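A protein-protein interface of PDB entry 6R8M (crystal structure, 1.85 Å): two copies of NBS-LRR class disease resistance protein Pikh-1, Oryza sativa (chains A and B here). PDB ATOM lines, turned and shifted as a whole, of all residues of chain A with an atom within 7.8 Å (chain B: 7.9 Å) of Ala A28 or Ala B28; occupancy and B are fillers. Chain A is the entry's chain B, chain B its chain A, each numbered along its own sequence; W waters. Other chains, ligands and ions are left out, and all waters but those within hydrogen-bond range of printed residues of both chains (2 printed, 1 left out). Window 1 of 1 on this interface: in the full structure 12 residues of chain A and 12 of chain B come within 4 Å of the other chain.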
ATOM      1  N   ARG A  20      22.829  21.068 -27.207  1.00  0.00           N
ATOM      2  CA  ARG A  20      21.523  20.970 -26.499  1.00  0.00           C
ATOM      3  C   ARG A  20      21.801  20.441 -25.093  1.00  0.00           C
ATOM      4  O   ARG A  20      21.242  20.970 -24.150  1.00  0.00           O
ATOM      5  CB  ARG A  20      20.519  20.115 -27.276  1.00  0.00           C
ATOM      6  CG  ARG A  20      20.007  20.785 -28.545  1.00  0.00           C
ATOM      7  CD  ARG A  20      18.846  20.002 -29.125  1.00  0.00           C
ATOM      8  NE  ARG A  20      19.244  18.863 -29.946  1.00  0.00           N
ATOM      9  CZ  ARG A  20      18.446  17.851 -30.292  1.00  0.00           C
ATOM     10  NH1 ARG A  20      17.194  17.797 -29.866  1.00  0.00           N
ATOM     11  NH2 ARG A  20      18.916  16.876 -31.054  1.00  0.00           N
ATOM     12  N   SER A  21      22.721  19.492 -24.974  1.00  0.00           N
ATOM     13  CA  SER A  21      23.160  18.901 -23.688  1.00  0.00           C
ATOM     14  C   SER A  21      23.867  19.939 -22.800  1.00  0.00           C
ATOM     15  O   SER A  21      23.593  20.010 -21.593  1.00  0.00           O
ATOM     16  CB  SER A  21      24.028  17.712 -23.964  1.00  0.00           C
ATOM     17  OG  SER A  21      24.341  17.061 -22.758  1.00  0.00           O
ATOM     18  N   LYS A  22      24.765  20.742 -23.351  1.00  0.00           N
ATOM     19  CA  LYS A  22      25.432  21.820 -22.576  1.00  0.00           C
ATOM     20  C   LYS A  22      24.391  22.883 -22.201  1.00  0.00           C
ATOM     21  O   LYS A  22      24.437  23.427 -21.100  1.00  0.00           O
ATOM     22  CB  LYS A  22      26.583  22.389 -23.413  1.00  0.00           C
ATOM     23  CG  LYS A  22      27.704  21.386 -23.686  1.00  0.00           C
ATOM     24  CD  LYS A  22      28.300  21.431 -25.096  1.00  0.00           C
ATOM     25  CE  LYS A  22      28.773  22.808 -25.518  1.00  0.00           C
ATOM     26  NZ  LYS A  22      29.478  23.515 -24.418  1.00  0.00           N
ATOM     27  N   ALA A  23      23.444  23.151 -23.085  1.00  0.00           N
ATOM     28  CA  ALA A  23      22.411  24.177 -22.834  1.00  0.00           C
ATOM     29  C   ALA A  23      21.549  23.695 -21.663  1.00  0.00           C
ATOM     30  O   ALA A  23      21.403  24.421 -20.681  1.00  0.00           O
ATOM     31  CB  ALA A  23      21.618  24.455 -24.103  1.00  0.00           C
ATOM     32  N   MET A  24      21.071  22.462 -21.746  1.00  0.00           N
ATOM     33  CA  MET A  24      20.232  21.849 -20.686  1.00  0.00           C
ATOM     34  C   MET A  24      20.980  21.907 -19.347  1.00  0.00           C
ATOM     35  O   MET A  24      20.400  22.294 -18.347  1.00  0.00           O
ATOM     36  CB  MET A  24      19.898  20.396 -21.045  1.00  0.00           C
ATOM     37  CG  MET A  24      18.980  20.258 -22.209  1.00  0.00           C
ATOM     38  SD  MET A  24      17.243  20.576 -21.724  1.00  0.00           S
ATOM     39  CE  MET A  24      16.863  19.047 -20.871  1.00  0.00           C
ATOM     40  N   ALA A  25      22.240  21.504 -19.310  1.00  0.00           N
ATOM     41  CA  ALA A  25      23.073  21.521 -18.090  1.00  0.00           C
ATOM     42  C   ALA A  25      23.189  22.940 -17.522  1.00  0.00           C
ATOM     43  O   ALA A  25      22.999  23.134 -16.313  1.00  0.00           O
ATOM     44  CB  ALA A  25      24.431  20.937 -18.425  1.00  0.00           C
ATOM     45  N   LEU A  26      23.481  23.927 -18.357  1.00  0.00           N
ATOM     46  CA  LEU A  26      23.628  25.336 -17.878  1.00  0.00           C
ATOM     47  C   LEU A  26      22.290  25.844 -17.311  1.00  0.00           C
ATOM     48  O   LEU A  26      22.238  26.295 -16.165  1.00  0.00           O
ATOM     49  CB  LEU A  26      24.087  26.208 -19.057  1.00  0.00           C
ATOM     50  CG  LEU A  26      24.332  27.684 -18.714  1.00  0.00           C
ATOM     51  CD1 LEU A  26      25.134  27.842 -17.442  1.00  0.00           C
ATOM     52  CD2 LEU A  26      25.040  28.397 -19.840  1.00  0.00           C
ATOM     53  N   VAL A  27      21.230  25.699 -18.084  1.00  0.00           N
ATOM     54  CA  VAL A  27      19.866  26.096 -17.632  1.00  0.00           C
ATOM     55  C   VAL A  27      19.526  25.355 -16.333  1.00  0.00           C
ATOM     56  O   VAL A  27      19.150  26.054 -15.360  1.00  0.00           O
ATOM     57  CB  VAL A  27      18.829  25.893 -18.738  1.00  0.00           C
ATOM     58  CG1 VAL A  27      17.416  26.196 -18.233  1.00  0.00           C
ATOM     59  CG2 VAL A  27      19.131  26.746 -19.958  1.00  0.00           C
ATOM     60  N   ALA A  28      19.742  24.028 -16.249  1.00  0.00           N
ATOM     61  CA  ALA A  28      19.321  23.229 -15.075  1.00  0.00           C
ATOM     62  C   ALA A  28      20.084  23.678 -13.823  1.00  0.00           C
ATOM     63  O   ALA A  28      19.545  23.528 -12.723  1.00  0.00           O
ATOM     64  CB  ALA A  28      19.513  21.750 -15.324  1.00  0.00           C
ATOM     65  N   SER A  29      21.305  24.185 -13.985  1.00  0.00           N
ATOM     66  CA  SER A  29      22.199  24.615 -12.877  1.00  0.00           C
ATOM     67  C   SER A  29      21.784  25.993 -12.337  1.00  0.00           C
ATOM     68  O   SER A  29      22.340  26.392 -11.324  1.00  0.00           O
ATOM     69  CB  SER A  29      23.651  24.652 -13.353  1.00  0.00           C
ATOM     70  OG  SER A  29      23.840  25.796 -14.172  1.00  0.00           O
ATOM     71  N   THR A  30      20.835  26.691 -12.958  1.00  0.00           N
ATOM     72  CA  THR A  30      20.468  28.076 -12.568  1.00  0.00           C
ATOM     73  C   THR A  30      19.551  28.097 -11.342  1.00  0.00           C
ATOM     74  O   THR A  30      18.649  27.245 -11.241  1.00  0.00           O
ATOM     75  CB  THR A  30      19.789  28.810 -13.720  1.00  0.00           C
ATOM     76  OG1 THR A  30      20.727  28.717 -14.788  1.00  0.00           O
ATOM     77  CG2 THR A  30      19.403  30.230 -13.351  1.00  0.00           C
ATOM     78  N   GLY A  31      19.749  29.074 -10.451  1.00  0.00           N
ATOM     79  CA  GLY A  31      18.983  29.190  -9.209  1.00  0.00           C
ATOM     80  C   GLY A  31      17.484  29.325  -9.501  1.00  0.00           C
ATOM     81  O   GLY A  31      17.148  29.993 -10.477  1.00  0.00           O
ATOM     82  N   GLY A  32      16.657  28.632  -8.714  1.00  0.00           N
ATOM     83  CA  GLY A  32      15.182  28.656  -8.763  1.00  0.00           C
ATOM     84  C   GLY A  32      14.593  27.811  -9.891  1.00  0.00           C
ATOM     85  O   GLY A  32      13.353  27.843 -10.054  1.00  0.00           O
ATOM     86  N   VAL A  33      15.398  27.041 -10.623  1.00  0.00           N
ATOM     87  CA  VAL A  33      14.882  26.167 -11.728  1.00  0.00           C
ATOM     88  C   VAL A  33      14.243  24.928 -11.121  1.00  0.00           C
ATOM     89  O   VAL A  33      14.927  24.210 -10.383  1.00  0.00           O
ATOM     90  CB  VAL A  33      15.969  25.791 -12.750  1.00  0.00           C
ATOM     91  CG1 VAL A  33      15.510  24.683 -13.701  1.00  0.00           C
ATOM     92  CG2 VAL A  33      16.460  26.992 -13.514  1.00  0.00           C
ATOM     93  N   ASP A  34      12.975  24.660 -11.444  1.00  0.00           N
ATOM     94  CA  ASP A  34      12.251  23.413 -11.069  1.00  0.00           C
ATOM     95  C   ASP A  34      12.423  22.347 -12.158  1.00  0.00           C
ATOM     96  O   ASP A  34      12.479  21.139 -11.821  1.00  0.00           O
ATOM     97  CB  ASP A  34      10.743  23.620 -10.899  1.00  0.00           C
ATOM     98  CG  ASP A  34      10.339  24.477  -9.707  1.00  0.00           C
ATOM     99  OD1 ASP A  34      11.202  24.721  -8.830  1.00  0.00           O
ATOM    100  OD2 ASP A  34       9.144  24.917  -9.679  1.00  0.00           O
ATOM    101  N   SER A  35      12.389  22.737 -13.422  1.00  0.00           N
ATOM    102  CA  SER A  35      12.472  21.771 -14.535  1.00  0.00           C
ATOM    103  C   SER A  35      13.034  22.414 -15.797  1.00  0.00           C
ATOM    104  O   SER A  35      12.904  23.617 -15.984  1.00  0.00           O
ATOM    105  CB  SER A  35      11.158  21.113 -14.789  1.00  0.00           C
ATOM    106  OG  SER A  35      10.208  22.022 -15.304  1.00  0.00           O
ATOM    107  N   VAL A  36      13.601  21.561 -16.633  1.00  0.00           N
ATOM    108  CA  VAL A  36      14.061  21.854 -18.001  1.00  0.00           C
ATOM    109  C   VAL A  36      13.605  20.710 -18.868  1.00  0.00           C
ATOM    110  O   VAL A  36      13.742  19.535 -18.455  1.00  0.00           O
ATOM    111  CB  VAL A  36      15.594  22.047 -18.101  1.00  0.00           C
ATOM    112  CG1 VAL A  36      15.996  23.291 -17.370  1.00  0.00           C
ATOM    113  CG2 VAL A  36      16.331  20.833 -17.558  1.00  0.00           C
ATOM    114  N   LEU A  38      13.405  19.592 -23.251  1.00  0.00           N
ATOM    115  CA  LEU A  38      13.605  19.775 -24.698  1.00  0.00           C
ATOM    116  C   LEU A  38      12.266  19.548 -25.343  1.00  0.00           C
ATOM    117  O   LEU A  38      11.775  18.439 -25.228  1.00  0.00           O
ATOM    118  CB  LEU A  38      14.623  18.763 -25.220  1.00  0.00           C
ATOM    119  CG  LEU A  38      16.054  19.148 -24.937  1.00  0.00           C
ATOM    120  CD1 LEU A  38      16.984  18.001 -25.292  1.00  0.00           C
ATOM    121  CD2 LEU A  38      16.405  20.411 -25.715  1.00  0.00           C
ATOM    122  N   ILE A  46      14.190  24.817 -25.165  1.00  0.00           N
ATOM    123  CA  ILE A  46      14.223  24.432 -23.742  1.00  0.00           C
ATOM    124  C   ILE A  46      13.086  25.199 -23.050  1.00  0.00           C
ATOM    125  O   ILE A  46      13.064  26.452 -23.068  1.00  0.00           O
ATOM    126  CB  ILE A  46      15.601  24.672 -23.106  1.00  0.00           C
ATOM    127  CG1 ILE A  46      16.696  23.909 -23.856  1.00  0.00           C
ATOM    128  CG2 ILE A  46      15.562  24.313 -21.627  1.00  0.00           C
ATOM    129  CD1 ILE A  46      18.096  24.112 -23.288  1.00  0.00           C
ATOM    130  N   VAL A  48      11.708  26.004 -19.468  1.00  0.00           N
ATOM    131  CA  VAL A  48      12.155  26.033 -18.049  1.00  0.00           C
ATOM    132  C   VAL A  48      10.999  26.540 -17.188  1.00  0.00           C
ATOM    133  O   VAL A  48      10.306  27.535 -17.556  1.00  0.00           O
ATOM    134  CB  VAL A  48      13.464  26.813 -17.792  1.00  0.00           C
ATOM    135  CG1 VAL A  48      13.366  28.271 -18.160  1.00  0.00           C
ATOM    136  CG2 VAL A  48      13.909  26.683 -16.345  1.00  0.00           C
ATOM    137  N   LEU A  58      19.857  34.784 -18.148  1.00  0.00           N
ATOM    138  CA  LEU A  58      19.954  33.357 -18.556  1.00  0.00           C
ATOM    139  C   LEU A  58      20.398  33.293 -20.022  1.00  0.00           C
ATOM    140  O   LEU A  58      21.263  32.499 -20.333  1.00  0.00           O
ATOM    141  CB  LEU A  58      18.586  32.689 -18.345  1.00  0.00           C
ATOM    142  CG  LEU A  58      18.511  31.190 -18.619  1.00  0.00           C
ATOM    143  CD1 LEU A  58      19.545  30.424 -17.824  1.00  0.00           C
ATOM    144  CD2 LEU A  58      17.125  30.654 -18.300  1.00  0.00           C
ATOM    145  N   ARG B  20      21.607  20.757  -5.288  1.00  0.00           N
ATOM    146  CA  ARG B  20      20.388  20.649  -6.144  1.00  0.00           C
ATOM    147  C   ARG B  20      20.736  21.090  -7.569  1.00  0.00           C
ATOM    148  O   ARG B  20      20.401  20.341  -8.514  1.00  0.00           O
ATOM    149  CB  ARG B  20      19.220  21.502  -5.633  1.00  0.00           C
ATOM    150  CG  ARG B  20      18.089  20.669  -5.045  1.00  0.00           C
ATOM    151  CD  ARG B  20      16.994  21.486  -4.387  1.00  0.00           C
ATOM    152  NE  ARG B  20      16.272  20.721  -3.373  1.00  0.00           N
ATOM    153  CZ  ARG B  20      16.716  20.435  -2.139  1.00  0.00           C
ATOM    154  NH1 ARG B  20      15.953  19.729  -1.321  1.00  0.00           N
ATOM    155  NH2 ARG B  20      17.907  20.842  -1.719  1.00  0.00           N
ATOM    156  N   SER B  21      21.386  22.252  -7.702  1.00  0.00           N
ATOM    157  CA  SER B  21      21.866  22.813  -8.992  1.00  0.00           C
ATOM    158  C   SER B  21      22.887  21.860  -9.640  1.00  0.00           C
ATOM    159  O   SER B  21      22.788  21.640 -10.857  1.00  0.00           O
ATOM    160  CB  SER B  21      22.417  24.195  -8.819  1.00  0.00           C
ATOM    161  OG  SER B  21      21.357  25.083  -8.514  1.00  0.00           O
ATOM    162  N   LYS B  22      23.809  21.299  -8.854  1.00  0.00           N
ATOM    163  CA  LYS B  22      24.851  20.351  -9.331  1.00  0.00           C
ATOM    164  C   LYS B  22      24.197  19.049  -9.823  1.00  0.00           C
ATOM    165  O   LYS B  22      24.566  18.557 -10.910  1.00  0.00           O
ATOM    166  CB  LYS B  22      25.854  20.069  -8.206  1.00  0.00           C
ATOM    167  CG  LYS B  22      26.754  21.250  -7.876  1.00  0.00           C
ATOM    168  CD  LYS B  22      27.510  21.144  -6.571  1.00  0.00           C
ATOM    169  CE  LYS B  22      28.700  22.086  -6.555  1.00  0.00           C
ATOM    170  NZ  LYS B  22      28.942  22.655  -5.210  1.00  0.00           N
ATOM    171  N   ALA B  23      23.298  18.461  -9.040  1.00  0.00           N
ATOM    172  CA  ALA B  23      22.612  17.212  -9.441  1.00  0.00           C
ATOM    173  C   ALA B  23      21.881  17.475 -10.763  1.00  0.00           C
ATOM    174  O   ALA B  23      22.018  16.684 -11.727  1.00  0.00           O
ATOM    175  CB  ALA B  23      21.658  16.772  -8.356  1.00  0.00           C
ATOM    176  N   MET B  24      21.119  18.561 -10.797  1.00  0.00           N
ATOM    177  CA  MET B  24      20.263  18.925 -11.950  1.00  0.00           C
ATOM    178  C   MET B  24      21.164  19.107 -13.170  1.00  0.00           C
ATOM    179  O   MET B  24      20.814  18.576 -14.208  1.00  0.00           O
ATOM    180  CB  MET B  24      19.447  20.191 -11.680  1.00  0.00           C
ATOM    181  CG  MET B  24      18.330  19.960 -10.666  1.00  0.00           C
ATOM    182  SD  MET B  24      16.975  19.020 -11.382  1.00  0.00           S
ATOM    183  CE  MET B  24      16.177  20.265 -12.398  1.00  0.00           C
ATOM    184  N   ALA B  25      22.291  19.812 -13.037  1.00  0.00           N
ATOM    185  CA  ALA B  25      23.215  20.043 -14.169  1.00  0.00           C
ATOM    186  C   ALA B  25      23.714  18.688 -14.688  1.00  0.00           C
ATOM    187  O   ALA B  25      23.655  18.469 -15.926  1.00  0.00           O
ATOM    188  CB  ALA B  25      24.350  20.939 -13.753  1.00  0.00           C
ATOM    189  N   LEU B  26      24.210  17.829 -13.788  1.00  0.00           N
ATOM    190  CA  LEU B  26      24.792  16.509 -14.142  1.00  0.00           C
ATOM    191  C   LEU B  26      23.731  15.654 -14.856  1.00  0.00           C
ATOM    192  O   LEU B  26      24.004  15.129 -15.947  1.00  0.00           O
ATOM    193  CB  LEU B  26      25.292  15.834 -12.864  1.00  0.00           C
ATOM    194  CG  LEU B  26      26.178  14.594 -13.044  1.00  0.00           C
ATOM    195  CD1 LEU B  26      26.737  14.129 -11.717  1.00  0.00           C
ATOM    196  CD2 LEU B  26      25.425  13.441 -13.672  1.00  0.00           C
ATOM    197  N   VAL B  27      22.548  15.519 -14.261  1.00  0.00           N
ATOM    198  CA  VAL B  27      21.439  14.738 -14.868  1.00  0.00           C
ATOM    199  C   VAL B  27      21.080  15.367 -16.211  1.00  0.00           C
ATOM    200  O   VAL B  27      21.092  14.643 -17.190  1.00  0.00           O
ATOM    201  CB  VAL B  27      20.231  14.627 -13.925  1.00  0.00           C
ATOM    202  CG1 VAL B  27      19.086  13.914 -14.614  1.00  0.00           C
ATOM    203  CG2 VAL B  27      20.597  13.937 -12.626  1.00  0.00           C
ATOM    204  N   ALA B  28      20.877  16.683 -16.283  1.00  0.00           N
ATOM    205  CA  ALA B  28      20.481  17.372 -17.528  1.00  0.00           C
ATOM    206  C   ALA B  28      21.553  17.210 -18.621  1.00  0.00           C
ATOM    207  O   ALA B  28      21.172  17.304 -19.768  1.00  0.00           O
ATOM    208  CB  ALA B  28      20.183  18.841 -17.271  1.00  0.00           C
ATOM    209  N   SER B  29      22.833  17.020 -18.287  1.00  0.00           N
ATOM    210  CA  SER B  29      23.931  16.876 -19.285  1.00  0.00           C
ATOM    211  C   SER B  29      23.996  15.431 -19.819  1.00  0.00           C
ATOM    212  O   SER B  29      24.763  15.182 -20.764  1.00  0.00           O
ATOM    213  CB  SER B  29      25.277  17.261 -18.663  1.00  0.00           C
ATOM    214  OG  SER B  29      25.670  16.258 -17.734  1.00  0.00           O
ATOM    215  N   THR B  30      23.292  14.484 -19.189  1.00  0.00           N
ATOM    216  CA  THR B  30      23.420  13.028 -19.446  1.00  0.00           C
ATOM    217  C   THR B  30      22.810  12.710 -20.804  1.00  0.00           C
ATOM    218  O   THR B  30      21.762  13.260 -21.148  1.00  0.00           O
ATOM    219  CB  THR B  30      22.733  12.214 -18.347  1.00  0.00           C
ATOM    220  OG1 THR B  30      23.331  12.594 -17.118  1.00  0.00           O
ATOM    221  CG2 THR B  30      22.790  10.713 -18.539  1.00  0.00           C
ATOM    222  N   GLY B  31      23.441  11.827 -21.563  1.00  0.00           N
ATOM    223  CA  GLY B  31      22.923  11.443 -22.882  1.00  0.00           C
ATOM    224  C   GLY B  31      21.565  10.778 -22.766  1.00  0.00           C
ATOM    225  O   GLY B  31      21.353   9.990 -21.810  1.00  0.00           O
ATOM    226  N   GLY B  32      20.703  11.043 -23.744  1.00  0.00           N
ATOM    227  CA  GLY B  32      19.338  10.492 -23.839  1.00  0.00           C
ATOM    228  C   GLY B  32      18.290  11.354 -23.130  1.00  0.00           C
ATOM    229  O   GLY B  32      17.096  11.095 -23.322  1.00  0.00           O
ATOM    230  N   VAL B  33      18.698  12.335 -22.320  1.00  0.00           N
ATOM    231  CA  VAL B  33      17.766  13.046 -21.388  1.00  0.00           C
ATOM    232  C   VAL B  33      16.949  14.081 -22.164  1.00  0.00           C
ATOM    233  O   VAL B  33      17.520  14.897 -22.868  1.00  0.00           O
ATOM    234  CB  VAL B  33      18.519  13.628 -20.185  1.00  0.00           C
ATOM    235  CG1 VAL B  33      17.661  14.609 -19.397  1.00  0.00           C
ATOM    236  CG2 VAL B  33      19.035  12.506 -19.300  1.00  0.00           C
ATOM    237  N   ASP B  34      15.610  13.987 -22.102  1.00  0.00           N
ATOM    238  CA  ASP B  34      14.674  14.990 -22.688  1.00  0.00           C
ATOM    239  C   ASP B  34      14.194  15.984 -21.625  1.00  0.00           C
ATOM    240  O   ASP B  34      13.994  17.184 -21.929  1.00  0.00           O
ATOM    241  CB  ASP B  34      13.472  14.304 -23.320  1.00  0.00           C
ATOM    242  CG  ASP B  34      13.774  13.581 -24.624  1.00  0.00           C
ATOM    243  OD1 ASP B  34      14.805  13.889 -25.255  1.00  0.00           O
ATOM    244  OD2 ASP B  34      12.976  12.723 -24.994  1.00  0.00           O
ATOM    245  N   SER B  35      13.948  15.527 -20.396  1.00  0.00           N
ATOM    246  CA  SER B  35      13.462  16.411 -19.329  1.00  0.00           C
ATOM    247  C   SER B  35      14.083  16.014 -18.011  1.00  0.00           C
ATOM    248  O   SER B  35      14.354  14.802 -17.782  1.00  0.00           O
ATOM    249  CB  SER B  35      11.953  16.418 -19.245  1.00  0.00           C
ATOM    250  OG  SER B  35      11.486  15.094 -19.018  1.00  0.00           O
ATOM    251  N   VAL B  36      14.265  17.019 -17.175  1.00  0.00           N
ATOM    252  CA  VAL B  36      14.636  16.882 -15.750  1.00  0.00           C
ATOM    253  C   VAL B  36      13.702  17.767 -14.929  1.00  0.00           C
ATOM    254  O   VAL B  36      13.607  18.984 -15.223  1.00  0.00           O
ATOM    255  CB  VAL B  36      16.098  17.280 -15.544  1.00  0.00           C
ATOM    256  CG1 VAL B  36      16.600  16.890 -14.164  1.00  0.00           C
ATOM    257  CG2 VAL B  36      16.956  16.710 -16.652  1.00  0.00           C
ATOM    258  N   LEU B  38      12.575  18.588 -10.604  1.00  0.00           N
ATOM    259  CA  LEU B  38      12.531  18.355  -9.144  1.00  0.00           C
ATOM    260  C   LEU B  38      11.094  18.019  -8.762  1.00  0.00           C
ATOM    261  O   LEU B  38      10.232  18.708  -9.230  1.00  0.00           O
ATOM    262  CB  LEU B  38      12.998  19.608  -8.415  1.00  0.00           C
ATOM    263  CG  LEU B  38      14.473  19.939  -8.563  1.00  0.00           C
ATOM    264  CD1 LEU B  38      14.792  21.325  -8.011  1.00  0.00           C
ATOM    265  CD2 LEU B  38      15.312  18.873  -7.888  1.00  0.00           C
ATOM    266  N   ILE B  46      14.578  13.780  -8.233  1.00  0.00           N
ATOM    267  CA  ILE B  46      14.769  14.229  -9.643  1.00  0.00           C
ATOM    268  C   ILE B  46      14.091  13.208 -10.541  1.00  0.00           C
ATOM    269  O   ILE B  46      14.378  11.995 -10.377  1.00  0.00           O
ATOM    270  CB  ILE B  46      16.245  14.423  -9.997  1.00  0.00           C
ATOM    271  CG1 ILE B  46      16.853  15.543  -9.157  1.00  0.00           C
ATOM    272  CG2 ILE B  46      16.393  14.711 -11.488  1.00  0.00           C
ATOM    273  CD1 ILE B  46      18.325  15.771  -9.405  1.00  0.00           C
ATOM    274  N   VAL B  48      13.716  12.120 -14.350  1.00  0.00           N
ATOM    275  CA  VAL B  48      14.497  12.161 -15.601  1.00  0.00           C
ATOM    276  C   VAL B  48      13.675  11.396 -16.621  1.00  0.00           C
ATOM    277  O   VAL B  48      13.329  10.240 -16.331  1.00  0.00           O
ATOM    278  CB  VAL B  48      15.868  11.490 -15.405  1.00  0.00           C
ATOM    279  CG1 VAL B  48      16.830  11.945 -16.492  1.00  0.00           C
ATOM    280  CG2 VAL B  48      16.387  11.793 -14.020  1.00  0.00           C
ATOM    281  N   LEU B  58      24.340   6.711 -14.524  1.00  0.00           N
ATOM    282  CA  LEU B  58      23.777   7.978 -13.997  1.00  0.00           C
ATOM    283  C   LEU B  58      23.918   7.969 -12.479  1.00  0.00           C
ATOM    284  O   LEU B  58      24.394   8.987 -11.909  1.00  0.00           O
ATOM    285  CB  LEU B  58      22.309   8.141 -14.409  1.00  0.00           C
ATOM    286  CG  LEU B  58      21.625   9.416 -13.925  1.00  0.00           C
ATOM    287  CD1 LEU B  58      22.502  10.644 -14.122  1.00  0.00           C
ATOM    288  CD2 LEU B  58      20.269   9.617 -14.629  1.00  0.00           C
ATOM    289  N   LEU B  62      26.246  10.352 -10.213  1.00  0.00           N
ATOM    290  CA  LEU B  62      25.649  11.244  -9.185  1.00  0.00           C
ATOM    291  C   LEU B  62      26.346  10.992  -7.841  1.00  0.00           C
ATOM    292  O   LEU B  62      26.574  11.979  -7.096  1.00  0.00           O
ATOM    293  CB  LEU B  62      24.148  11.017  -9.032  1.00  0.00           C
ATOM    294  CG  LEU B  62      23.230  11.815  -9.961  1.00  0.00           C
ATOM    295  CD1 LEU B  62      21.829  11.260  -9.854  1.00  0.00           C
ATOM    296  CD2 LEU B  62      23.217  13.302  -9.651  1.00  0.00           C
HETATM  297  O   HOH W   1       9.292  20.480 -11.059  1.00  0.00           O
HETATM  298  O   HOH W   2      19.130  24.792 -10.301  1.00  0.00           O
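OG of Ser A21 lies within hydrogen-bond range of O of Ser B29 (2.8 Å). The backbone carbonyl oxygen (O) of Asp B34 is in hydrogen-bond range of the backbone NH (N) of Leu A38 (2.8 Å). The backbone carbonyl oxygen (O) of Val A36 is in hydrogen-bond range of the backbone NH (N) of Val B36 (2.9 Å). N of Leu B38 lies within hydrogen-bond range of O of Asp A34 (2.8 Å). OG of Ser B21 lies within hydrogen-bond range of O of Ser A29, at 3.3 Å.
OG of Ser B29 lies close to O of Ala B25 (3.5 Å). OG of Ser B29 lies within hydrogen-bond range of O of Leu B26. The side-chain hydroxyl (OG) of Ser A29 is in hydrogen-bond range of the backbone carbonyl oxygen (O) of Leu A26, at 2.6 Å.
Met A24 touches Ala B28. CE of Met A24 touches O of Asp B34 (3.6 Å). O of Ala B25 touches CB of Ala A25, at 3.6 Å. Ala B28 touches Ala A25. Ala A25 touches Ser B29 (CB to CB, 3.8 Å). Met B24 touches Ala A28. Ala B25 touches Ser A29. Val A33 touches Leu B38 (O to CD1, 3.7 Å). Met B24 touches Asp A34 (CE to O, 3.8 Å). Val B36 touches Ser A35.
Of chain B, only Met B24 (3.5 Å) and Ala B28 (3.6 Å) come within 4 Å of Ala A28. Ala B28 touches just these residues of chain A: Met A24 (3.6 Å), Ala A25 (3.9 Å) and Ala A28 (3.6 Å). Printed residues of chain A within 4 Å of Met B24: Ala A28 (3.5 Å) and Asp A34 (3.8 Å). Printed residues of chain B within 4 Å of Val A36: Ser B35 and Val B36. Of the printed residues of chain B, Met A24 touches Ala B28 (3.6 Å) and Asp B34 (3.6 Å). Printed residues of chain A within 4 Å of Ser B21: Ser A29 (3.3 Å). Of the printed residues of chain B, Ala A25 touches Ala B25, Ala B28 and Ser B29. The nearest printed residue of chain B that does not touch Leu A38 is Ser B35 (5.0 Å).
Of the 21 printed residues of chain A, 10 touch a printed residue of chain B. Of the 22 printed residues of chain B, 10 touch a printed residue of chain A. Hydrophobic or aromatic side chains of chain B within 4 Å of the printed part of chain A: Met B24, Ala B25, Ala B28 and Leu B38. Among the printed residues, 18 pairs touch across the chains. Among the printed residues, no Asp or Glu carboxylate lies within 4 Å of a Lys or Arg side-chain nitrogen of the other chain.
Ser A21 touches Ser B29, and with the chains exchanged Ser A29 touches Ser B21. Met A24 touches Ala B28, and with the chains exchanged Ala A28 touches Met B24. Ala A28 touches its own counterpart, Ala B28. Val A33 touches Leu B38, and with the chains exchanged Leu A38 touches Val B33. 21 positions are printed for both chains. Of the 18 pairs that touch across the chains among the printed residues, 17 have their exchanged pair printed and touching as well.
Water W2 lies within hydrogen-bond range of the backbone carbonyl oxygen (O) of Thr A30 (2.7 Å), the backbone carbonyl oxygen (O) of Ala A28 (2.8 Å) and the side-chain hydroxyl (OG) of Ser B21 (2.9 Å). Water W1 lies within hydrogen-bond range of O of Leu B38 (2.7 Å) and O of Asp A34 (3.3 Å).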
